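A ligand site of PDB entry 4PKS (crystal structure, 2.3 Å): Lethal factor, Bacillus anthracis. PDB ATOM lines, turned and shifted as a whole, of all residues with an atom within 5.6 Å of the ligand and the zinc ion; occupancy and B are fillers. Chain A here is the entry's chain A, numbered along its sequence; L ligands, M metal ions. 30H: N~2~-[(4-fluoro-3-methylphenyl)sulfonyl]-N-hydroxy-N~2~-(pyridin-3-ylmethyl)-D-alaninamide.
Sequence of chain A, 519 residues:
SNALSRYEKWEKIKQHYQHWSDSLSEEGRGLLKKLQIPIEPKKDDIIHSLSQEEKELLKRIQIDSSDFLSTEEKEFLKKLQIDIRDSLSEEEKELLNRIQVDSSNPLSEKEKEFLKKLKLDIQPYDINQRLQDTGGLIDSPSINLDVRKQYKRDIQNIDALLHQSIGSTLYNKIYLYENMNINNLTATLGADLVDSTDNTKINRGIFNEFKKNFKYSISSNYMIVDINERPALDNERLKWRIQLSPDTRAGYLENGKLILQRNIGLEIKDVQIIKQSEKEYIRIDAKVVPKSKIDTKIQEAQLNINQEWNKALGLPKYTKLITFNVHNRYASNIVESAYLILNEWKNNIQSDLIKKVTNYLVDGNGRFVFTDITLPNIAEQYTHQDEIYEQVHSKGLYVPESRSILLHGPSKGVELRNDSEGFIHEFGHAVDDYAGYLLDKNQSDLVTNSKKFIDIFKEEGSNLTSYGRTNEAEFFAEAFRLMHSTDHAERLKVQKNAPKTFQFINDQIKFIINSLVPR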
ATOM      1  N   ASP A  67       1.111  10.445  -6.280  1.00  0.00           N
ATOM      2  CA  ASP A  67       0.745  11.761  -6.799  1.00  0.00           C
ATOM      3  C   ASP A  67       1.416  12.082  -8.134  1.00  0.00           C
ATOM      4  O   ASP A  67       0.866  12.852  -8.922  1.00  0.00           O
ATOM      5  CB  ASP A  67       1.116  12.843  -5.776  1.00  0.00           C
ATOM      6  CG  ASP A  67       0.153  12.897  -4.607  1.00  0.00           C
ATOM      7  OD1 ASP A  67      -0.787  12.086  -4.562  1.00  0.00           O
ATOM      8  OD2 ASP A  67       0.338  13.770  -3.731  1.00  0.00           O
ATOM      9  N   PHE A  68       2.584  11.502  -8.373  1.00  0.00           N
ATOM     10  CA  PHE A  68       3.400  11.915  -9.508  1.00  0.00           C
ATOM     11  C   PHE A  68       3.553  10.886 -10.627  1.00  0.00           C
ATOM     12  O   PHE A  68       4.494  10.958 -11.412  1.00  0.00           O
ATOM     13  CB  PHE A  68       4.796  12.311  -9.026  1.00  0.00           C
ATOM     14  CG  PHE A  68       4.903  13.741  -8.581  1.00  0.00           C
ATOM     15  CD1 PHE A  68       3.821  14.372  -7.984  1.00  0.00           C
ATOM     16  CD2 PHE A  68       6.064  14.457  -8.774  1.00  0.00           C
ATOM     17  CE1 PHE A  68       3.913  15.683  -7.564  1.00  0.00           C
ATOM     18  CE2 PHE A  68       6.168  15.769  -8.376  1.00  0.00           C
ATOM     19  CZ  PHE A  68       5.082  16.381  -7.768  1.00  0.00           C
ATOM     20  N   VAL A 392      11.180  17.258 -11.908  1.00  0.00           N
ATOM     21  CA  VAL A 392       9.726  17.279 -11.777  1.00  0.00           C
ATOM     22  C   VAL A 392       9.061  17.897 -13.003  1.00  0.00           C
ATOM     23  O   VAL A 392       9.481  18.945 -13.487  1.00  0.00           O
ATOM     24  CB  VAL A 392       9.292  18.071 -10.516  1.00  0.00           C
ATOM     25  CG1 VAL A 392       7.781  18.278 -10.492  1.00  0.00           C
ATOM     26  CG2 VAL A 392       9.756  17.357  -9.255  1.00  0.00           C
ATOM     27  N   SER A 394       5.218  19.268 -14.039  1.00  0.00           N
ATOM     28  CA  SER A 394       3.916  19.623 -13.492  1.00  0.00           C
ATOM     29  C   SER A 394       3.396  20.888 -14.155  1.00  0.00           C
ATOM     30  O   SER A 394       4.038  21.426 -15.058  1.00  0.00           O
ATOM     31  CB  SER A 394       4.005  19.796 -11.971  1.00  0.00           C
ATOM     32  OG  SER A 394       5.082  20.658 -11.614  1.00  0.00           O
ATOM     33  N   LYS A 395       2.236  21.362 -13.704  1.00  0.00           N
ATOM     34  CA  LYS A 395       1.679  22.612 -14.205  1.00  0.00           C
ATOM     35  C   LYS A 395       2.605  23.773 -13.889  1.00  0.00           C
ATOM     36  O   LYS A 395       2.889  24.607 -14.763  1.00  0.00           O
ATOM     37  CB  LYS A 395       0.289  22.851 -13.597  1.00  0.00           C
ATOM     38  CG  LYS A 395      -0.149  24.309 -13.558  1.00  0.00           C
ATOM     39  CD  LYS A 395      -0.343  24.885 -14.960  1.00  0.00           C
ATOM     40  CE  LYS A 395      -1.467  24.174 -15.688  1.00  0.00           C
ATOM     41  NZ  LYS A 395      -1.646  24.737 -17.063  1.00  0.00           N
ATOM     42  N   GLY A 396       3.088  23.821 -12.664  1.00  0.00           N
ATOM     43  CA  GLY A 396       3.938  24.910 -12.224  1.00  0.00           C
ATOM     44  C   GLY A 396       5.051  24.438 -11.309  1.00  0.00           C
ATOM     45  O   GLY A 396       4.957  23.366 -10.699  1.00  0.00           O
ATOM     46  N   LEU A 397       6.108  25.230 -11.213  1.00  0.00           N
ATOM     47  CA  LEU A 397       7.249  24.890 -10.379  1.00  0.00           C
ATOM     48  C   LEU A 397       8.014  26.138  -9.951  1.00  0.00           C
ATOM     49  O   LEU A 397       8.020  27.148 -10.649  1.00  0.00           O
ATOM     50  CB  LEU A 397       8.180  23.933 -11.119  1.00  0.00           C
ATOM     51  CG  LEU A 397       9.241  23.226 -10.276  1.00  0.00           C
ATOM     52  CD1 LEU A 397       8.570  22.360  -9.223  1.00  0.00           C
ATOM     53  CD2 LEU A 397      10.179  22.407 -11.145  1.00  0.00           C
ATOM     54  N   TYR A 398       8.659  26.062  -8.786  1.00  0.00           N
ATOM     55  CA  TYR A 398       9.600  27.089  -8.362  1.00  0.00           C
ATOM     56  C   TYR A 398      10.960  26.475  -8.032  1.00  0.00           C
ATOM     57  O   TYR A 398      11.036  25.494  -7.300  1.00  0.00           O
ATOM     58  CB  TYR A 398       9.067  27.865  -7.161  1.00  0.00           C
ATOM     59  CG  TYR A 398      10.054  28.903  -6.677  1.00  0.00           C
ATOM     60  CD1 TYR A 398      10.253  30.079  -7.386  1.00  0.00           C
ATOM     61  CD2 TYR A 398      10.810  28.690  -5.533  1.00  0.00           C
ATOM     62  CE1 TYR A 398      11.162  31.023  -6.953  1.00  0.00           C
ATOM     63  CE2 TYR A 398      11.733  29.625  -5.101  1.00  0.00           C
ATOM     64  CZ  TYR A 398      11.896  30.785  -5.812  1.00  0.00           C
ATOM     65  OH  TYR A 398      12.805  31.729  -5.379  1.00  0.00           O
ATOM     66  N   GLY A 413      -3.322  21.386 -13.765  1.00  0.00           N
ATOM     67  CA  GLY A 413      -2.935  21.140 -12.384  1.00  0.00           C
ATOM     68  C   GLY A 413      -4.013  20.417 -11.605  1.00  0.00           C
ATOM     69  O   GLY A 413      -5.191  20.755 -11.696  1.00  0.00           O
ATOM     70  N   VAL A 414      -3.610  19.398 -10.848  1.00  0.00           N
ATOM     71  CA  VAL A 414      -4.546  18.616 -10.056  1.00  0.00           C
ATOM     72  C   VAL A 414      -5.201  19.475  -8.979  1.00  0.00           C
ATOM     73  O   VAL A 414      -4.504  20.108  -8.179  1.00  0.00           O
ATOM     74  CB  VAL A 414      -3.865  17.408  -9.390  1.00  0.00           C
ATOM     75  CG1 VAL A 414      -4.893  16.566  -8.650  1.00  0.00           C
ATOM     76  CG2 VAL A 414      -3.137  16.575 -10.435  1.00  0.00           C
ATOM     77  N   GLU A 415      -6.525  19.492  -8.976  1.00  0.00           N
ATOM     78  CA  GLU A 415      -7.312  20.328  -8.053  1.00  0.00           C
ATOM     79  C   GLU A 415      -6.887  21.785  -8.160  1.00  0.00           C
ATOM     80  O   GLU A 415      -6.566  22.433  -7.160  1.00  0.00           O
ATOM     81  CB  GLU A 415      -7.162  19.829  -6.619  1.00  0.00           C
ATOM     82  CG  GLU A 415      -8.164  18.742  -6.244  1.00  0.00           C
ATOM     83  CD  GLU A 415      -7.583  17.687  -5.327  1.00  0.00           C
ATOM     84  OE1 GLU A 415      -6.943  16.746  -5.838  1.00  0.00           O
ATOM     85  OE2 GLU A 415      -7.760  17.817  -4.093  1.00  0.00           O
ATOM     86  N   LEU A 416      -6.879  22.288  -9.393  1.00  0.00           N
ATOM     87  CA  LEU A 416      -6.474  23.663  -9.677  1.00  0.00           C
ATOM     88  C   LEU A 416      -7.385  24.250 -10.752  1.00  0.00           C
ATOM     89  O   LEU A 416      -7.515  23.678 -11.840  1.00  0.00           O
ATOM     90  CB  LEU A 416      -5.018  23.712 -10.120  1.00  0.00           C
ATOM     91  CG  LEU A 416      -4.374  25.091 -10.288  1.00  0.00           C
ATOM     92  CD1 LEU A 416      -4.241  25.772  -8.933  1.00  0.00           C
ATOM     93  CD2 LEU A 416      -3.024  24.960 -10.958  1.00  0.00           C
ATOM     94  N   GLU A 421      -4.027  30.795 -10.764  1.00  0.00           N
ATOM     95  CA  GLU A 421      -3.973  30.253  -9.408  1.00  0.00           C
ATOM     96  C   GLU A 421      -2.699  29.443  -9.201  1.00  0.00           C
ATOM     97  O   GLU A 421      -2.120  29.437  -8.120  1.00  0.00           O
ATOM     98  CB  GLU A 421      -5.204  29.399  -9.107  1.00  0.00           C
ATOM     99  CG  GLU A 421      -6.500  30.191  -9.044  1.00  0.00           C
ATOM    100  CD  GLU A 421      -7.630  29.408  -8.417  1.00  0.00           C
ATOM    101  OE1 GLU A 421      -7.512  28.162  -8.333  1.00  0.00           O
ATOM    102  OE2 GLU A 421      -8.622  30.031  -7.986  1.00  0.00           O
ATOM    103  N   GLY A 422      -2.265  28.752 -10.254  1.00  0.00           N
ATOM    104  CA  GLY A 422      -1.034  27.993 -10.198  1.00  0.00           C
ATOM    105  C   GLY A 422       0.163  28.909 -10.025  1.00  0.00           C
ATOM    106  O   GLY A 422       1.053  28.631  -9.218  1.00  0.00           O
ATOM    107  N   HIS A 425       0.478  30.233  -6.520  1.00  0.00           N
ATOM    108  CA  HIS A 425       1.062  29.185  -5.695  1.00  0.00           C
ATOM    109  C   HIS A 425       2.586  29.173  -5.796  1.00  0.00           C
ATOM    110  O   HIS A 425       3.283  29.125  -4.784  1.00  0.00           O
ATOM    111  CB  HIS A 425       0.481  27.826  -6.110  1.00  0.00           C
ATOM    112  CG  HIS A 425       1.142  26.642  -5.456  1.00  0.00           C
ATOM    113  ND1 HIS A 425       0.542  25.928  -4.444  1.00  0.00           N
ATOM    114  CD2 HIS A 425       2.313  26.028  -5.707  1.00  0.00           C
ATOM    115  CE1 HIS A 425       1.332  24.928  -4.097  1.00  0.00           C
ATOM    116  NE2 HIS A 425       2.413  24.967  -4.836  1.00  0.00           N
ATOM    117  N   GLU A 426       3.092  29.216  -7.024  1.00  0.00           N
ATOM    118  CA  GLU A 426       4.545  29.237  -7.235  1.00  0.00           C
ATOM    119  C   GLU A 426       5.163  30.501  -6.641  1.00  0.00           C
ATOM    120  O   GLU A 426       6.286  30.475  -6.153  1.00  0.00           O
ATOM    121  CB  GLU A 426       4.883  29.152  -8.734  1.00  0.00           C
ATOM    122  CG  GLU A 426       4.138  28.071  -9.508  1.00  0.00           C
ATOM    123  CD  GLU A 426       4.328  26.674  -8.931  1.00  0.00           C
ATOM    124  OE1 GLU A 426       3.428  25.830  -9.127  1.00  0.00           O
ATOM    125  OE2 GLU A 426       5.373  26.417  -8.299  1.00  0.00           O
ATOM    126  N   HIS A 429       6.026  30.081  -3.081  1.00  0.00           N
ATOM    127  CA  HIS A 429       7.358  29.504  -2.875  1.00  0.00           C
ATOM    128  C   HIS A 429       8.441  30.573  -2.909  1.00  0.00           C
ATOM    129  O   HIS A 429       9.400  30.507  -2.134  1.00  0.00           O
ATOM    130  CB  HIS A 429       7.661  28.445  -3.949  1.00  0.00           C
ATOM    131  CG  HIS A 429       6.875  27.179  -3.793  1.00  0.00           C
ATOM    132  ND1 HIS A 429       6.791  26.496  -2.602  1.00  0.00           N
ATOM    133  CD2 HIS A 429       6.155  26.459  -4.692  1.00  0.00           C
ATOM    134  CE1 HIS A 429       6.050  25.412  -2.769  1.00  0.00           C
ATOM    135  NE2 HIS A 429       5.655  25.367  -4.030  1.00  0.00           N
ATOM    136  N   TYR A 467      -3.280  18.216  -0.928  1.00  0.00           N
ATOM    137  CA  TYR A 467      -1.904  18.282  -1.397  1.00  0.00           C
ATOM    138  C   TYR A 467      -1.042  19.157  -0.481  1.00  0.00           C
ATOM    139  O   TYR A 467       0.184  19.000  -0.434  1.00  0.00           O
ATOM    140  CB  TYR A 467      -1.832  18.794  -2.828  1.00  0.00           C
ATOM    141  CG  TYR A 467      -0.419  18.933  -3.322  1.00  0.00           C
ATOM    142  CD1 TYR A 467       0.369  17.813  -3.522  1.00  0.00           C
ATOM    143  CD2 TYR A 467       0.142  20.177  -3.539  1.00  0.00           C
ATOM    144  CE1 TYR A 467       1.672  17.921  -3.956  1.00  0.00           C
ATOM    145  CE2 TYR A 467       1.446  20.310  -3.977  1.00  0.00           C
ATOM    146  CZ  TYR A 467       2.206  19.179  -4.179  1.00  0.00           C
ATOM    147  OH  TYR A 467       3.504  19.300  -4.612  1.00  0.00           O
ATOM    148  N   GLU A 474       4.993  23.134   0.486  1.00  0.00           N
ATOM    149  CA  GLU A 474       3.755  23.004  -0.262  1.00  0.00           C
ATOM    150  C   GLU A 474       2.561  23.503   0.550  1.00  0.00           C
ATOM    151  O   GLU A 474       1.630  24.080   0.003  1.00  0.00           O
ATOM    152  CB  GLU A 474       3.529  21.546  -0.690  1.00  0.00           C
ATOM    153  CG  GLU A 474       4.334  21.087  -1.914  1.00  0.00           C
ATOM    154  CD  GLU A 474       4.531  22.167  -2.973  1.00  0.00           C
ATOM    155  OE1 GLU A 474       3.553  22.880  -3.314  1.00  0.00           O
ATOM    156  OE2 GLU A 474       5.662  22.283  -3.472  1.00  0.00           O
ATOM    157  N   ALA A 477       2.727  27.298   0.408  1.00  0.00           N
ATOM    158  CA  ALA A 477       2.346  27.814  -0.904  1.00  0.00           C
ATOM    159  C   ALA A 477       0.860  27.657  -1.164  1.00  0.00           C
ATOM    160  O   ALA A 477       0.240  28.521  -1.788  1.00  0.00           O
ATOM    161  CB  ALA A 477       3.142  27.115  -1.992  1.00  0.00           C
ATOM    162  N   GLU A 478       0.278  26.559  -0.689  1.00  0.00           N
ATOM    163  CA  GLU A 478      -1.154  26.324  -0.803  1.00  0.00           C
ATOM    164  C   GLU A 478      -1.929  27.332   0.031  1.00  0.00           C
ATOM    165  O   GLU A 478      -2.917  27.904  -0.431  1.00  0.00           O
ATOM    166  CB  GLU A 478      -1.506  24.904  -0.383  1.00  0.00           C
ATOM    167  CG  GLU A 478      -1.251  23.856  -1.454  1.00  0.00           C
ATOM    168  CD  GLU A 478      -2.163  24.037  -2.655  1.00  0.00           C
ATOM    169  OE1 GLU A 478      -3.255  23.427  -2.674  1.00  0.00           O
ATOM    170  OE2 GLU A 478      -1.790  24.792  -3.583  1.00  0.00           O
ATOM    171  N   ARG A 481      -1.833  30.637  -1.623  1.00  0.00           N
ATOM    172  CA  ARG A 481      -2.719  30.666  -2.775  1.00  0.00           C
ATOM    173  C   ARG A 481      -4.152  30.963  -2.358  1.00  0.00           C
ATOM    174  O   ARG A 481      -4.797  31.851  -2.907  1.00  0.00           O
ATOM    175  CB  ARG A 481      -2.671  29.331  -3.533  1.00  0.00           C
ATOM    176  CG  ARG A 481      -3.673  29.243  -4.682  1.00  0.00           C
ATOM    177  CD  ARG A 481      -3.538  27.967  -5.488  1.00  0.00           C
ATOM    178  NE  ARG A 481      -3.850  26.765  -4.713  1.00  0.00           N
ATOM    179  CZ  ARG A 481      -5.073  26.289  -4.540  1.00  0.00           C
ATOM    180  NH1 ARG A 481      -6.117  26.903  -5.076  1.00  0.00           N
ATOM    181  NH2 ARG A 481      -5.260  25.185  -3.814  1.00  0.00           N
HETATM  182  O4  30H L   1       3.984  21.934  -6.358  1.00  0.00           O
HETATM  183  C6  30H L   1       4.450  19.798  -8.250  1.00  0.00           C
HETATM  184  C11 30H L   1       1.739  19.981  -7.400  1.00  0.00           C
HETATM  185  C12 30H L   1       1.123  18.643  -7.741  1.00  0.00           C
HETATM  186  C13 30H L   1       1.598  17.849  -8.773  1.00  0.00           C
HETATM  187  C14 30H L   1       0.980  16.633  -9.010  1.00  0.00           C
HETATM  188  C15 30H L   1      -0.099  16.234  -8.225  1.00  0.00           C
HETATM  189  C17 30H L   1       0.051  18.203  -6.976  1.00  0.00           C
HETATM  190  C18 30H L   1       0.466  22.574  -8.847  1.00  0.00           C
HETATM  191  C19 30H L   1      -0.661  22.297  -8.086  1.00  0.00           C
HETATM  192  C20 30H L   1      -1.344  23.324  -7.435  1.00  0.00           C
HETATM  193  C1  30H L   1       4.027  22.130  -7.558  1.00  0.00           C
HETATM  194  C2  30H L   1       3.638  21.058  -8.544  1.00  0.00           C
HETATM  195  N3  30H L   1       4.435  23.292  -8.060  1.00  0.00           N
HETATM  196  O5  30H L   1       5.175  24.166  -7.259  1.00  0.00           O
HETATM  197  N7  30H L   1       2.202  20.789  -8.535  1.00  0.00           N
HETATM  198  S8  30H L   1       1.240  21.387  -9.572  1.00  0.00           S
HETATM  199  O9  30H L   1       0.293  20.411 -10.046  1.00  0.00           O
HETATM  200  O10 30H L   1       1.986  21.892 -10.693  1.00  0.00           O
HETATM  201  N16 30H L   1      -0.537  17.024  -7.228  1.00  0.00           N
HETATM  202  C21 30H L   1      -0.891  24.633  -7.557  1.00  0.00           C
HETATM  203  C22 30H L   1       0.233  24.917  -8.323  1.00  0.00           C
HETATM  204  C23 30H L   1       0.916  23.891  -8.975  1.00  0.00           C
HETATM  205  F24 30H L   1      -1.556  25.617  -6.933  1.00  0.00           F
HETATM  206  C25 30H L   1      -2.563  23.023  -6.614  1.00  0.00           C
HETATM  207 ZN    ZN M   1       4.485  23.745  -5.045  1.00  0.00          ZN
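Within 4 Å of the zinc ion: His 425, His 429 and Glu 474. The nearest printed residue that does not touch the zinc ion is Glu 426 (4.3 Å).
The side-chain hydroxyl (OG) of Ser 394 sits close to an oxygen (O10) of the ligand (3.5 Å). The backbone carbonyl oxygen of Gly 396 is in hydrogen-bond range of a nitrogen (N3) of the ligand (2.7 Å). An oxygen (O10) of the ligand lies within hydrogen-bond range of the backbone NH of Gly 396, 3.0 Å away. The side-chain hydroxyl of Tyr 467 sits close to an oxygen (O4) of the ligand. OE1 of Glu 426 lies within hydrogen-bond range of N3 of the ligand, 2.9 Å away. An oxygen (O10) of the ligand is in hydrogen-bond range of the backbone NH (N) of Lys 395, 3.1 Å away.
OE1 of Glu 474 is bound to the zinc ion (2.1 Å). A ring nitrogen (NE2) of His 429 binds the zinc ion. O4 of the ligand is bound to the zinc ion, 2.3 Å away. An oxygen (O5) of the ligand binds the zinc ion (2.4 Å). A ring nitrogen (NE2) of His 425 binds the zinc ion (2.4 Å). OE2 of Glu 474 binds the zinc ion (2.4 Å). The zinc ion has six donor atoms within binding distance.
The side-chain carboxylate (OE2) of Glu 478 lies close to a fluorine (F24) of the ligand. The guanidinium group (NE) of Arg 481 lies close to a fluorine (F24) of the ligand (3.4 Å). Residues that only touch the ligand: Leu 416, Phe 68, Asp 67, Val 414, Leu 397 and Gly 422. 16 residues have an atom within 4 Å of the ligand: Asp 67, Phe 68, Ser 394, Lys 395, Gly 396, Leu 397, Val 414, Leu 416, Gly 422, His 425, Glu 426, His 429, Tyr 467, Glu 474, Glu 478 and Arg 481. Along chain A the residues within 4 Å of the ligand span positions 67 to 481. The nearest printed residue that does not touch the ligand is Glu 421 (4.04 Å).
NH1 of Arg 481 is in salt-bridge range of OE1 of Glu 421, 3.8 Å away. The side-chain hydroxyl (OG) of Ser 394 is in hydrogen-bond range of the backbone carbonyl oxygen (O) of Gly 396 (2.9 Å). ND1 of His 425 is in hydrogen-bond range of OE2 of Glu 478 (2.7 Å). N of Leu 397 lies close to OE2 of Glu 426 (3.2 Å). NH2 of Arg 481 lies within salt-bridge range of OE1 of Glu 478 (2.9 Å). N of Tyr 398 sits at hydrogen-bond distance from OE2 of Glu 426 (3.3 Å).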
